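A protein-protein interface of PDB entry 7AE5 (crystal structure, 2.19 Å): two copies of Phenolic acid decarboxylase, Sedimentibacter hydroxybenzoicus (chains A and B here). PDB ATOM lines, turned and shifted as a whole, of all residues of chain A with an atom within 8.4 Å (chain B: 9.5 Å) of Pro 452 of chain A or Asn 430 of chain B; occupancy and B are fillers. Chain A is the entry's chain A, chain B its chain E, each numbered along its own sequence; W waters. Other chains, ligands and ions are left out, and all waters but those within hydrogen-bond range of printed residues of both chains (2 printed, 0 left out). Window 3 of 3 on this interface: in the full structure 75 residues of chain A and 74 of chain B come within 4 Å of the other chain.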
ATOM      1  N   THR A 406      17.658 -16.436  -9.140  1.00  0.00           N
ATOM      2  CA  THR A 406      17.793 -15.671  -7.909  1.00  0.00           C
ATOM      3  C   THR A 406      17.787 -16.506  -6.632  1.00  0.00           C
ATOM      4  O   THR A 406      18.139 -15.971  -5.576  1.00  0.00           O
ATOM      5  CB  THR A 406      16.677 -14.616  -7.808  1.00  0.00           C
ATOM      6  OG1 THR A 406      15.402 -15.269  -7.770  1.00  0.00           O
ATOM      7  CG2 THR A 406      16.719 -13.673  -9.001  1.00  0.00           C
ATOM      8  N   VAL A 408      18.916 -20.080  -6.567  1.00  0.00           N
ATOM      9  CA  VAL A 408      19.795 -21.237  -6.691  1.00  0.00           C
ATOM     10  C   VAL A 408      21.228 -20.763  -6.503  1.00  0.00           C
ATOM     11  O   VAL A 408      21.761 -20.016  -7.331  1.00  0.00           O
ATOM     12  CB  VAL A 408      19.630 -21.940  -8.044  1.00  0.00           C
ATOM     13  CG1 VAL A 408      20.695 -23.019  -8.209  1.00  0.00           C
ATOM     14  CG2 VAL A 408      18.246 -22.534  -8.172  1.00  0.00           C
ATOM     15  N   HIS A 409      21.847 -21.189  -5.411  1.00  0.00           N
ATOM     16  CA  HIS A 409      23.295 -21.134  -5.290  1.00  0.00           C
ATOM     17  C   HIS A 409      23.815 -22.478  -5.781  1.00  0.00           C
ATOM     18  O   HIS A 409      23.713 -23.479  -5.061  1.00  0.00           O
ATOM     19  CB  HIS A 409      23.724 -20.859  -3.849  1.00  0.00           C
ATOM     20  CG  HIS A 409      25.200 -20.673  -3.679  1.00  0.00           C
ATOM     21  ND1 HIS A 409      26.122 -21.628  -4.050  1.00  0.00           N
ATOM     22  CD2 HIS A 409      25.914 -19.639  -3.173  1.00  0.00           C
ATOM     23  CE1 HIS A 409      27.339 -21.192  -3.781  1.00  0.00           C
ATOM     24  NE2 HIS A 409      27.241 -19.987  -3.247  1.00  0.00           N
ATOM     25  N   PRO A 410      24.351 -22.549  -7.003  1.00  0.00           N
ATOM     26  CA  PRO A 410      24.713 -23.857  -7.572  1.00  0.00           C
ATOM     27  C   PRO A 410      25.762 -24.609  -6.774  1.00  0.00           C
ATOM     28  O   PRO A 410      25.913 -25.821  -6.971  1.00  0.00           O
ATOM     29  CB  PRO A 410      25.222 -23.496  -8.974  1.00  0.00           C
ATOM     30  CG  PRO A 410      24.552 -22.187  -9.278  1.00  0.00           C
ATOM     31  CD  PRO A 410      24.559 -21.459  -7.968  1.00  0.00           C
ATOM     32  N   GLY A 411      26.490 -23.938  -5.880  1.00  0.00           N
ATOM     33  CA  GLY A 411      27.424 -24.638  -5.018  1.00  0.00           C
ATOM     34  C   GLY A 411      26.763 -25.453  -3.926  1.00  0.00           C
ATOM     35  O   GLY A 411      27.425 -26.299  -3.315  1.00  0.00           O
ATOM     36  N   LYS A 412      25.477 -25.221  -3.668  1.00  0.00           N
ATOM     37  CA  LYS A 412      24.776 -25.929  -2.601  1.00  0.00           C
ATOM     38  C   LYS A 412      23.341 -26.315  -2.936  1.00  0.00           C
ATOM     39  O   LYS A 412      22.872 -27.334  -2.419  1.00  0.00           O
ATOM     40  CB  LYS A 412      24.775 -25.090  -1.314  1.00  0.00           C
ATOM     41  CG  LYS A 412      23.898 -23.844  -1.376  1.00  0.00           C
ATOM     42  CD  LYS A 412      23.777 -23.171  -0.016  1.00  0.00           C
ATOM     43  CE  LYS A 412      22.772 -22.026  -0.057  1.00  0.00           C
ATOM     44  NZ  LYS A 412      21.392 -22.491  -0.396  1.00  0.00           N
ATOM     45  N   ASP A 413      22.624 -25.556  -3.769  1.00  0.00           N
ATOM     46  CA  ASP A 413      21.236 -25.856  -4.105  1.00  0.00           C
ATOM     47  C   ASP A 413      21.092 -26.933  -5.182  1.00  0.00           C
ATOM     48  O   ASP A 413      19.959 -27.312  -5.495  1.00  0.00           O
ATOM     49  CB  ASP A 413      20.507 -24.581  -4.571  1.00  0.00           C
ATOM     50  CG  ASP A 413      19.884 -23.770  -3.421  1.00  0.00           C
ATOM     51  OD1 ASP A 413      19.115 -24.322  -2.608  1.00  0.00           O
ATOM     52  OD2 ASP A 413      20.117 -22.545  -3.359  1.00  0.00           O
ATOM     53  N   THR A 444      13.712 -20.163  -1.457  1.00  0.00           N
ATOM     54  CA  THR A 444      14.285 -19.153  -0.580  1.00  0.00           C
ATOM     55  C   THR A 444      14.608 -19.772   0.775  1.00  0.00           C
ATOM     56  O   THR A 444      13.750 -20.437   1.363  1.00  0.00           O
ATOM     57  CB  THR A 444      13.298 -18.005  -0.394  1.00  0.00           C
ATOM     58  OG1 THR A 444      12.896 -17.502  -1.675  1.00  0.00           O
ATOM     59  CG2 THR A 444      13.911 -16.885   0.424  1.00  0.00           C
ATOM     60  N   PRO A 445      15.816 -19.568   1.299  1.00  0.00           N
ATOM     61  CA  PRO A 445      16.182 -20.186   2.579  1.00  0.00           C
ATOM     62  C   PRO A 445      15.263 -19.756   3.713  1.00  0.00           C
ATOM     63  O   PRO A 445      14.858 -18.595   3.809  1.00  0.00           O
ATOM     64  CB  PRO A 445      17.615 -19.696   2.802  1.00  0.00           C
ATOM     65  CG  PRO A 445      18.141 -19.501   1.410  1.00  0.00           C
ATOM     66  CD  PRO A 445      16.972 -18.932   0.646  1.00  0.00           C
ATOM     67  N   GLU A 449      18.555 -22.574   7.850  1.00  0.00           N
ATOM     68  CA  GLU A 449      19.522 -22.344   6.781  1.00  0.00           C
ATOM     69  C   GLU A 449      19.894 -20.867   6.745  1.00  0.00           C
ATOM     70  O   GLU A 449      19.002 -20.010   6.739  1.00  0.00           O
ATOM     71  CB  GLU A 449      18.972 -22.774   5.423  1.00  0.00           C
ATOM     72  CG  GLU A 449      19.893 -22.396   4.267  1.00  0.00           C
ATOM     73  CD  GLU A 449      19.365 -22.828   2.913  1.00  0.00           C
ATOM     74  OE1 GLU A 449      18.290 -23.463   2.863  1.00  0.00           O
ATOM     75  OE2 GLU A 449      20.027 -22.529   1.895  1.00  0.00           O
ATOM     76  N   PRO A 450      21.180 -20.528   6.734  1.00  0.00           N
ATOM     77  CA  PRO A 450      21.564 -19.115   6.705  1.00  0.00           C
ATOM     78  C   PRO A 450      21.170 -18.462   5.392  1.00  0.00           C
ATOM     79  O   PRO A 450      21.147 -19.093   4.333  1.00  0.00           O
ATOM     80  CB  PRO A 450      23.090 -19.153   6.870  1.00  0.00           C
ATOM     81  CG  PRO A 450      23.398 -20.523   7.390  1.00  0.00           C
ATOM     82  CD  PRO A 450      22.348 -21.418   6.816  1.00  0.00           C
ATOM     83  N   ASN A 451      20.846 -17.177   5.477  1.00  0.00           N
ATOM     84  CA  ASN A 451      20.514 -16.389   4.296  1.00  0.00           C
ATOM     85  C   ASN A 451      21.638 -15.399   4.034  1.00  0.00           C
ATOM     86  O   ASN A 451      21.873 -14.506   4.866  1.00  0.00           O
ATOM     87  CB  ASN A 451      19.185 -15.657   4.483  1.00  0.00           C
ATOM     88  CG  ASN A 451      18.536 -15.281   3.165  1.00  0.00           C
ATOM     89  OD1 ASN A 451      19.188 -14.754   2.265  1.00  0.00           O
ATOM     90  ND2 ASN A 451      17.243 -15.555   3.047  1.00  0.00           N
ATOM     91  N   PRO A 452      22.362 -15.513   2.917  1.00  0.00           N
ATOM     92  CA  PRO A 452      23.439 -14.548   2.644  1.00  0.00           C
ATOM     93  C   PRO A 452      22.942 -13.118   2.540  1.00  0.00           C
ATOM     94  O   PRO A 452      23.690 -12.184   2.855  1.00  0.00           O
ATOM     95  CB  PRO A 452      24.025 -15.045   1.315  1.00  0.00           C
ATOM     96  CG  PRO A 452      22.927 -15.854   0.692  1.00  0.00           C
ATOM     97  CD  PRO A 452      22.214 -16.504   1.839  1.00  0.00           C
ATOM     98  N   ARG A 453      21.697 -12.925   2.110  1.00  0.00           N
ATOM     99  CA  ARG A 453      21.075 -11.610   2.030  1.00  0.00           C
ATOM    100  C   ARG A 453      19.575 -11.781   1.844  1.00  0.00           C
ATOM    101  O   ARG A 453      19.123 -12.152   0.756  1.00  0.00           O
ATOM    102  CB  ARG A 453      21.666 -10.789   0.883  1.00  0.00           C
ATOM    103  CG  ARG A 453      21.025  -9.421   0.710  1.00  0.00           C
ATOM    104  CD  ARG A 453      21.856  -8.522  -0.193  1.00  0.00           C
ATOM    105  NE  ARG A 453      21.722  -8.882  -1.600  1.00  0.00           N
ATOM    106  CZ  ARG A 453      20.690  -8.553  -2.364  1.00  0.00           C
ATOM    107  NH1 ARG A 453      19.673  -7.853  -1.889  1.00  0.00           N
ATOM    108  NH2 ARG A 453      20.678  -8.932  -3.639  1.00  0.00           N
ATOM    109  N   GLU A 454      18.793 -11.537   2.892  1.00  0.00           N
ATOM    110  CA  GLU A 454      17.352 -11.720   2.816  1.00  0.00           C
ATOM    111  C   GLU A 454      16.700 -10.452   2.276  1.00  0.00           C
ATOM    112  O   GLU A 454      17.012  -9.339   2.717  1.00  0.00           O
ATOM    113  CB  GLU A 454      16.769 -12.119   4.175  1.00  0.00           C
ATOM    114  CG  GLU A 454      16.576 -11.010   5.196  1.00  0.00           C
ATOM    115  CD  GLU A 454      16.269 -11.553   6.580  1.00  0.00           C
ATOM    116  OE1 GLU A 454      15.470 -12.510   6.677  1.00  0.00           O
ATOM    117  OE2 GLU A 454      16.822 -11.026   7.571  1.00  0.00           O
ATOM    118  N   THR A 455      15.826 -10.626   1.292  1.00  0.00           N
ATOM    119  CA  THR A 455      15.154  -9.528   0.622  1.00  0.00           C
ATOM    120  C   THR A 455      13.660  -9.591   0.899  1.00  0.00           C
ATOM    121  O   THR A 455      13.107 -10.659   1.177  1.00  0.00           O
ATOM    122  CB  THR A 455      15.391  -9.574  -0.892  1.00  0.00           C
ATOM    123  OG1 THR A 455      14.818 -10.774  -1.428  1.00  0.00           O
ATOM    124  CG2 THR A 455      16.879  -9.548  -1.202  1.00  0.00           C
ATOM    125  N   LYS B 383      24.784 -16.826 -14.520  1.00  0.00           N
ATOM    126  CA  LYS B 383      25.022 -17.914 -13.581  1.00  0.00           C
ATOM    127  C   LYS B 383      24.631 -19.272 -14.141  1.00  0.00           C
ATOM    128  O   LYS B 383      25.379 -20.242 -13.986  1.00  0.00           O
ATOM    129  CB  LYS B 383      24.253 -17.660 -12.278  1.00  0.00           C
ATOM    130  CG  LYS B 383      24.411 -18.752 -11.228  1.00  0.00           C
ATOM    131  CD  LYS B 383      23.778 -18.341  -9.907  1.00  0.00           C
ATOM    132  CE  LYS B 383      22.271 -18.184 -10.040  1.00  0.00           C
ATOM    133  NZ  LYS B 383      21.655 -17.574  -8.826  1.00  0.00           N
ATOM    134  N   GLU B 418      33.079 -22.949  -9.116  1.00  0.00           N
ATOM    135  CA  GLU B 418      33.017 -22.033  -7.987  1.00  0.00           C
ATOM    136  C   GLU B 418      33.998 -20.876  -8.153  1.00  0.00           C
ATOM    137  O   GLU B 418      34.906 -20.910  -8.987  1.00  0.00           O
ATOM    138  CB  GLU B 418      33.314 -22.768  -6.681  1.00  0.00           C
ATOM    139  CG  GLU B 418      32.328 -23.867  -6.349  1.00  0.00           C
ATOM    140  CD  GLU B 418      32.142 -24.042  -4.857  1.00  0.00           C
ATOM    141  OE1 GLU B 418      33.136 -24.365  -4.167  1.00  0.00           O
ATOM    142  OE2 GLU B 418      31.002 -23.849  -4.375  1.00  0.00           O
ATOM    143  N   ASN B 419      33.790 -19.840  -7.339  1.00  0.00           N
ATOM    144  CA  ASN B 419      34.714 -18.709  -7.231  1.00  0.00           C
ATOM    145  C   ASN B 419      34.853 -17.961  -8.555  1.00  0.00           C
ATOM    146  O   ASN B 419      35.957 -17.622  -8.986  1.00  0.00           O
ATOM    147  CB  ASN B 419      36.079 -19.168  -6.716  1.00  0.00           C
ATOM    148  CG  ASN B 419      36.845 -18.057  -6.035  1.00  0.00           C
ATOM    149  OD1 ASN B 419      36.313 -17.371  -5.163  1.00  0.00           O
ATOM    150  ND2 ASN B 419      38.105 -17.879  -6.420  1.00  0.00           N
ATOM    151  N   CYS B 420      33.725 -17.700  -9.202  1.00  0.00           N
ATOM    152  CA  CYS B 420      33.643 -16.931 -10.431  1.00  0.00           C
ATOM    153  C   CYS B 420      33.017 -15.569 -10.160  1.00  0.00           C
ATOM    154  O   CYS B 420      32.409 -15.360  -9.105  1.00  0.00           O
ATOM    155  CB  CYS B 420      32.807 -17.680 -11.477  1.00  0.00           C
ATOM    156  SG  CYS B 420      33.528 -19.225 -12.029  1.00  0.00           S
ATOM    157  N   GLY B 422      30.426 -12.593  -9.906  1.00  0.00           N
ATOM    158  CA  GLY B 422      28.989 -12.550  -9.745  1.00  0.00           C
ATOM    159  C   GLY B 422      28.488 -11.127  -9.630  1.00  0.00           C
ATOM    160  O   GLY B 422      29.264 -10.178  -9.771  1.00  0.00           O
ATOM    161  N   MET B 423      27.193 -10.964  -9.379  1.00  0.00           N
ATOM    162  CA  MET B 423      26.627  -9.645  -9.172  1.00  0.00           C
ATOM    163  C   MET B 423      25.862  -9.622  -7.857  1.00  0.00           C
ATOM    164  O   MET B 423      25.124 -10.565  -7.549  1.00  0.00           O
ATOM    165  CB  MET B 423      25.697  -9.251 -10.328  1.00  0.00           C
ATOM    166  CG  MET B 423      26.428  -8.860 -11.601  1.00  0.00           C
ATOM    167  SD  MET B 423      27.026  -7.158 -11.602  1.00  0.00           S
ATOM    168  CE  MET B 423      28.724  -7.361 -11.071  1.00  0.00           C
ATOM    169  N   PRO B 424      26.026  -8.564  -7.061  1.00  0.00           N
ATOM    170  CA  PRO B 424      25.345  -8.520  -5.758  1.00  0.00           C
ATOM    171  C   PRO B 424      23.834  -8.599  -5.856  1.00  0.00           C
ATOM    172  O   PRO B 424      23.198  -9.145  -4.945  1.00  0.00           O
ATOM    173  CB  PRO B 424      25.798  -7.174  -5.172  1.00  0.00           C
ATOM    174  CG  PRO B 424      27.074  -6.863  -5.871  1.00  0.00           C
ATOM    175  CD  PRO B 424      26.936  -7.423  -7.255  1.00  0.00           C
ATOM    176  N   ASP B 426      22.032 -10.520  -7.325  1.00  0.00           N
ATOM    177  CA  ASP B 426      21.611 -11.900  -7.126  1.00  0.00           C
ATOM    178  C   ASP B 426      21.684 -12.186  -5.631  1.00  0.00           C
ATOM    179  O   ASP B 426      22.784 -12.310  -5.077  1.00  0.00           O
ATOM    180  CB  ASP B 426      22.495 -12.863  -7.925  1.00  0.00           C
ATOM    181  CG  ASP B 426      22.098 -14.325  -7.748  1.00  0.00           C
ATOM    182  OD1 ASP B 426      21.107 -14.615  -7.043  1.00  0.00           O
ATOM    183  OD2 ASP B 426      22.786 -15.192  -8.325  1.00  0.00           O
ATOM    184  N   PRO B 427      20.543 -12.293  -4.945  1.00  0.00           N
ATOM    185  CA  PRO B 427      20.582 -12.398  -3.478  1.00  0.00           C
ATOM    186  C   PRO B 427      21.073 -13.741  -2.976  1.00  0.00           C
ATOM    187  O   PRO B 427      21.433 -13.845  -1.797  1.00  0.00           O
ATOM    188  CB  PRO B 427      19.123 -12.151  -3.077  1.00  0.00           C
ATOM    189  CG  PRO B 427      18.340 -12.667  -4.238  1.00  0.00           C
ATOM    190  CD  PRO B 427      19.170 -12.386  -5.471  1.00  0.00           C
ATOM    191  N   SER B 428      21.108 -14.766  -3.826  1.00  0.00           N
ATOM    192  CA  SER B 428      21.561 -16.086  -3.411  1.00  0.00           C
ATOM    193  C   SER B 428      23.077 -16.236  -3.443  1.00  0.00           C
ATOM    194  O   SER B 428      23.584 -17.286  -3.032  1.00  0.00           O
ATOM    195  CB  SER B 428      20.920 -17.158  -4.295  1.00  0.00           C
ATOM    196  OG  SER B 428      21.348 -17.029  -5.640  1.00  0.00           O
ATOM    197  N   THR B 429      23.807 -15.227  -3.915  1.00  0.00           N
ATOM    198  CA  THR B 429      25.259 -15.323  -3.980  1.00  0.00           C
ATOM    199  C   THR B 429      25.856 -15.436  -2.583  1.00  0.00           C
ATOM    200  O   THR B 429      25.471 -14.711  -1.662  1.00  0.00           O
ATOM    201  CB  THR B 429      25.844 -14.110  -4.706  1.00  0.00           C
ATOM    202  OG1 THR B 429      25.398 -12.905  -4.069  1.00  0.00           O
ATOM    203  CG2 THR B 429      25.411 -14.102  -6.165  1.00  0.00           C
ATOM    204  N   ASN B 430      26.801 -16.360  -2.430  1.00  0.00           N
ATOM    205  CA  ASN B 430      27.481 -16.586  -1.156  1.00  0.00           C
ATOM    206  C   ASN B 430      28.874 -17.112  -1.470  1.00  0.00           C
ATOM    207  O   ASN B 430      29.032 -18.285  -1.842  1.00  0.00           O
ATOM    208  CB  ASN B 430      26.715 -17.562  -0.266  1.00  0.00           C
ATOM    209  CG  ASN B 430      27.108 -17.456   1.196  1.00  0.00           C
ATOM    210  OD1 ASN B 430      28.066 -16.765   1.543  1.00  0.00           O
ATOM    211  ND2 ASN B 430      26.370 -18.143   2.062  1.00  0.00           N
ATOM    212  N   PRO B 431      29.919 -16.278  -1.336  1.00  0.00           N
ATOM    213  CA  PRO B 431      29.930 -14.889  -0.855  1.00  0.00           C
ATOM    214  C   PRO B 431      29.174 -13.925  -1.765  1.00  0.00           C
ATOM    215  O   PRO B 431      29.163 -14.124  -2.979  1.00  0.00           O
ATOM    216  CB  PRO B 431      31.424 -14.534  -0.834  1.00  0.00           C
ATOM    217  CG  PRO B 431      32.150 -15.838  -0.952  1.00  0.00           C
ATOM    218  CD  PRO B 431      31.261 -16.717  -1.749  1.00  0.00           C
ATOM    219  N   PRO B 432      28.535 -12.915  -1.178  1.00  0.00           N
ATOM    220  CA  PRO B 432      27.797 -11.938  -1.987  1.00  0.00           C
ATOM    221  C   PRO B 432      28.689 -11.318  -3.053  1.00  0.00           C
ATOM    222  O   PRO B 432      29.830 -10.932  -2.790  1.00  0.00           O
ATOM    223  CB  PRO B 432      27.339 -10.903  -0.955  1.00  0.00           C
ATOM    224  CG  PRO B 432      27.274 -11.661   0.331  1.00  0.00           C
ATOM    225  CD  PRO B 432      28.391 -12.666   0.267  1.00  0.00           C
ATOM    226  N   GLY B 433      28.165 -11.243  -4.276  1.00  0.00           N
ATOM    227  CA  GLY B 433      28.906 -10.711  -5.396  1.00  0.00           C
ATOM    228  C   GLY B 433      29.777 -11.713  -6.123  1.00  0.00           C
ATOM    229  O   GLY B 433      30.368 -11.363  -7.151  1.00  0.00           O
ATOM    230  N   MET B 434      29.891 -12.937  -5.615  1.00  0.00           N
ATOM    231  CA  MET B 434      30.597 -14.013  -6.292  1.00  0.00           C
ATOM    232  C   MET B 434      29.594 -15.053  -6.768  1.00  0.00           C
ATOM    233  O   MET B 434      28.528 -15.233  -6.171  1.00  0.00           O
ATOM    234  CB  MET B 434      31.635 -14.670  -5.375  1.00  0.00           C
ATOM    235  CG  MET B 434      32.672 -13.707  -4.824  1.00  0.00           C
ATOM    236  SD  MET B 434      33.882 -13.208  -6.063  1.00  0.00           S
ATOM    237  CE  MET B 434      34.592 -14.796  -6.495  1.00  0.00           C
ATOM    238  N   HIS B 435      29.939 -15.736  -7.852  1.00  0.00           N
ATOM    239  CA  HIS B 435      29.060 -16.730  -8.442  1.00  0.00           C
ATOM    240  C   HIS B 435      29.724 -18.096  -8.441  1.00  0.00           C
ATOM    241  O   HIS B 435      30.947 -18.220  -8.572  1.00  0.00           O
ATOM    242  CB  HIS B 435      28.677 -16.367  -9.885  1.00  0.00           C
ATOM    243  CG  HIS B 435      27.337 -15.713 -10.015  1.00  0.00           C
ATOM    244  ND1 HIS B 435      26.967 -14.994 -11.132  1.00  0.00           N
ATOM    245  CD2 HIS B 435      26.279 -15.667  -9.171  1.00  0.00           C
ATOM    246  CE1 HIS B 435      25.739 -14.534 -10.970  1.00  0.00           C
ATOM    247  NE2 HIS B 435      25.299 -14.928  -9.788  1.00  0.00           N
ATOM    248  N   THR B 436      28.899 -19.118  -8.279  1.00  0.00           N
ATOM    249  CA  THR B 436      29.242 -20.472  -8.681  1.00  0.00           C
ATOM    250  C   THR B 436      28.468 -20.744  -9.965  1.00  0.00           C
ATOM    251  O   THR B 436      27.242 -20.884  -9.940  1.00  0.00           O
ATOM    252  CB  THR B 436      28.902 -21.481  -7.590  1.00  0.00           C
ATOM    253  OG1 THR B 436      29.782 -21.285  -6.476  1.00  0.00           O
ATOM    254  CG2 THR B 436      29.080 -22.885  -8.112  1.00  0.00           C
HETATM  255  O   HOH W   1      27.687 -17.494  -4.787  1.00  0.00           O
HETATM  256  O   HOH W   2      24.081 -10.314  -2.652  1.00  0.00           O
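The side-chain amino group (NZ) of Lys 383 of chain B sits at hydrogen-bond distance from the backbone carbonyl oxygen (O) of Val 408 of chain A (2.9 Å).
The backbone carbonyl oxygen (O) of Pro 424 of chain B sits at hydrogen-bond distance from the guanidinium group (NH2) of Arg 453 of chain A.
The side-chain hydroxyl (OG) of Ser 428 of chain B sits close to the backbone carbonyl oxygen (O) of Thr 406 of chain A, 3.4 Å away.
OG of Ser 428 of chain B sits at hydrogen-bond distance from O of Val 408 of chain A.
A ring nitrogen (NE2) of His 409 of chain A lies within hydrogen-bond range of the backbone carbonyl oxygen (O) of Asn 430 of chain B (2.8 Å).
The side-chain amino group (NZ) of Lys 383 of chain B lies within salt-bridge range of the side-chain carboxylate (OD2) of Asp 426 of chain B (2.7 Å).
OD1 of Asp 426 of chain B sits at hydrogen-bond distance from OG of Ser 428 of chain B, at 2.8 Å.
The backbone carbonyl oxygen (O) of Asp 426 of chain B lies within hydrogen-bond range of the side-chain hydroxyl (OG1) of Thr 429 of chain B (2.9 Å).
The side-chain hydroxyl (OG1) of Thr 429 of chain B sits at hydrogen-bond distance from the backbone NH (N) of Gly 433 of chain B (3.2 Å).
N of His 409 of chain A is in hydrogen-bond range of OD2 of Asp 413 of chain A (3.0 Å).
The side-chain amide oxygen (OD1) of Asn 451 of chain A sits close to the backbone carbonyl oxygen (O) of Arg 453 of chain A, at 3.0 Å.
Among the printed residues, pairs that only touch across the chains: Thr 406 of chain A with Asp 426 of chain B, Thr 406 of chain A with Pro 427 of chain B, His 409 of chain A with Ser 428 of chain B, His 409 of chain A with Thr 436 of chain B, Pro 410 of chain A with Lys 383 of chain B, Pro 410 of chain A with Thr 436 of chain B, Gly 411 of chain A with Glu 418 of chain B, Gly 411 of chain A with Thr 436 of chain B, Pro 452 of chain A with Pro 427 of chain B, Pro 452 of chain A with Thr 429 of chain B, Pro 452 of chain A with Asn 430 of chain B, Arg 453 of chain A with Asp 426 of chain B, Arg 453 of chain A with Pro 427 of chain B and Thr 455 of chain A with Pro 427 of chain B.
Of chain A, only His 409 and Pro 452 come within 4 Å of Asn 430 of chain B.
No residue of chain B comes within 4 Å of Asn 451 of chain A.
No residue of chain A comes within 4 Å of Pro 431 of chain B.
Printed residues of chain A within 4 Å of Glu 418 of chain B: Gly 411.
Printed residues of chain B within 4 Å of Arg 453 of chain A: Pro 424 (2.8 Å), Asp 426 (3.9 Å) and Pro 427 (3.5 Å).
Printed residues of chain A within 4 Å of Lys 383 of chain B: Val 408 and Pro 410.
Of the printed residues of chain A, Asp 426 of chain B touches Thr 406 and Arg 453.
Thr 444 of chain A touches none of the printed residues of chain B.
The nearest residue of chain B that does not touch Pro 452 of chain A is Ser 428 of chain B (4.04 Å).
The nearest residue of chain A that does not touch Asn 430 of chain B is Lys 412 of chain A (5.7 Å).
The nearest printed residue of chain A that does not touch Thr 436 of chain B is Val 408 of chain A (6.1 Å).
Of the 16 printed residues of chain A, 8 touch a printed residue of chain B.
Printed residues of chain A that touch a printed residue of chain B: Thr 406, Val 408, His 409, Pro 410, Gly 411, Pro 452, Arg 453 and Thr 455.
Hydrophobic or aromatic side chains of chain A that line the printed part of chain B: His 409, Pro 410 and Pro 452.
Among the printed residues, no Asp or Glu carboxylate lies within 4 Å of a Lys or Arg side-chain nitrogen of the other chain.
No position is printed for both chains.
Water W2 lies within hydrogen-bond range of O of Pro 424 of chain B, NE of Arg 453 of chain A, OG1 of Thr 429 of chain B and O of Asp 426 of chain B.
Water W1 lies within hydrogen-bond range of the backbone NH of Asn 430 of chain B (2.8 Å), the backbone carbonyl oxygen of Met 434 of chain B (2.8 Å) and a ring nitrogen (NE2) of His 409 of chain A (3.0 Å).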
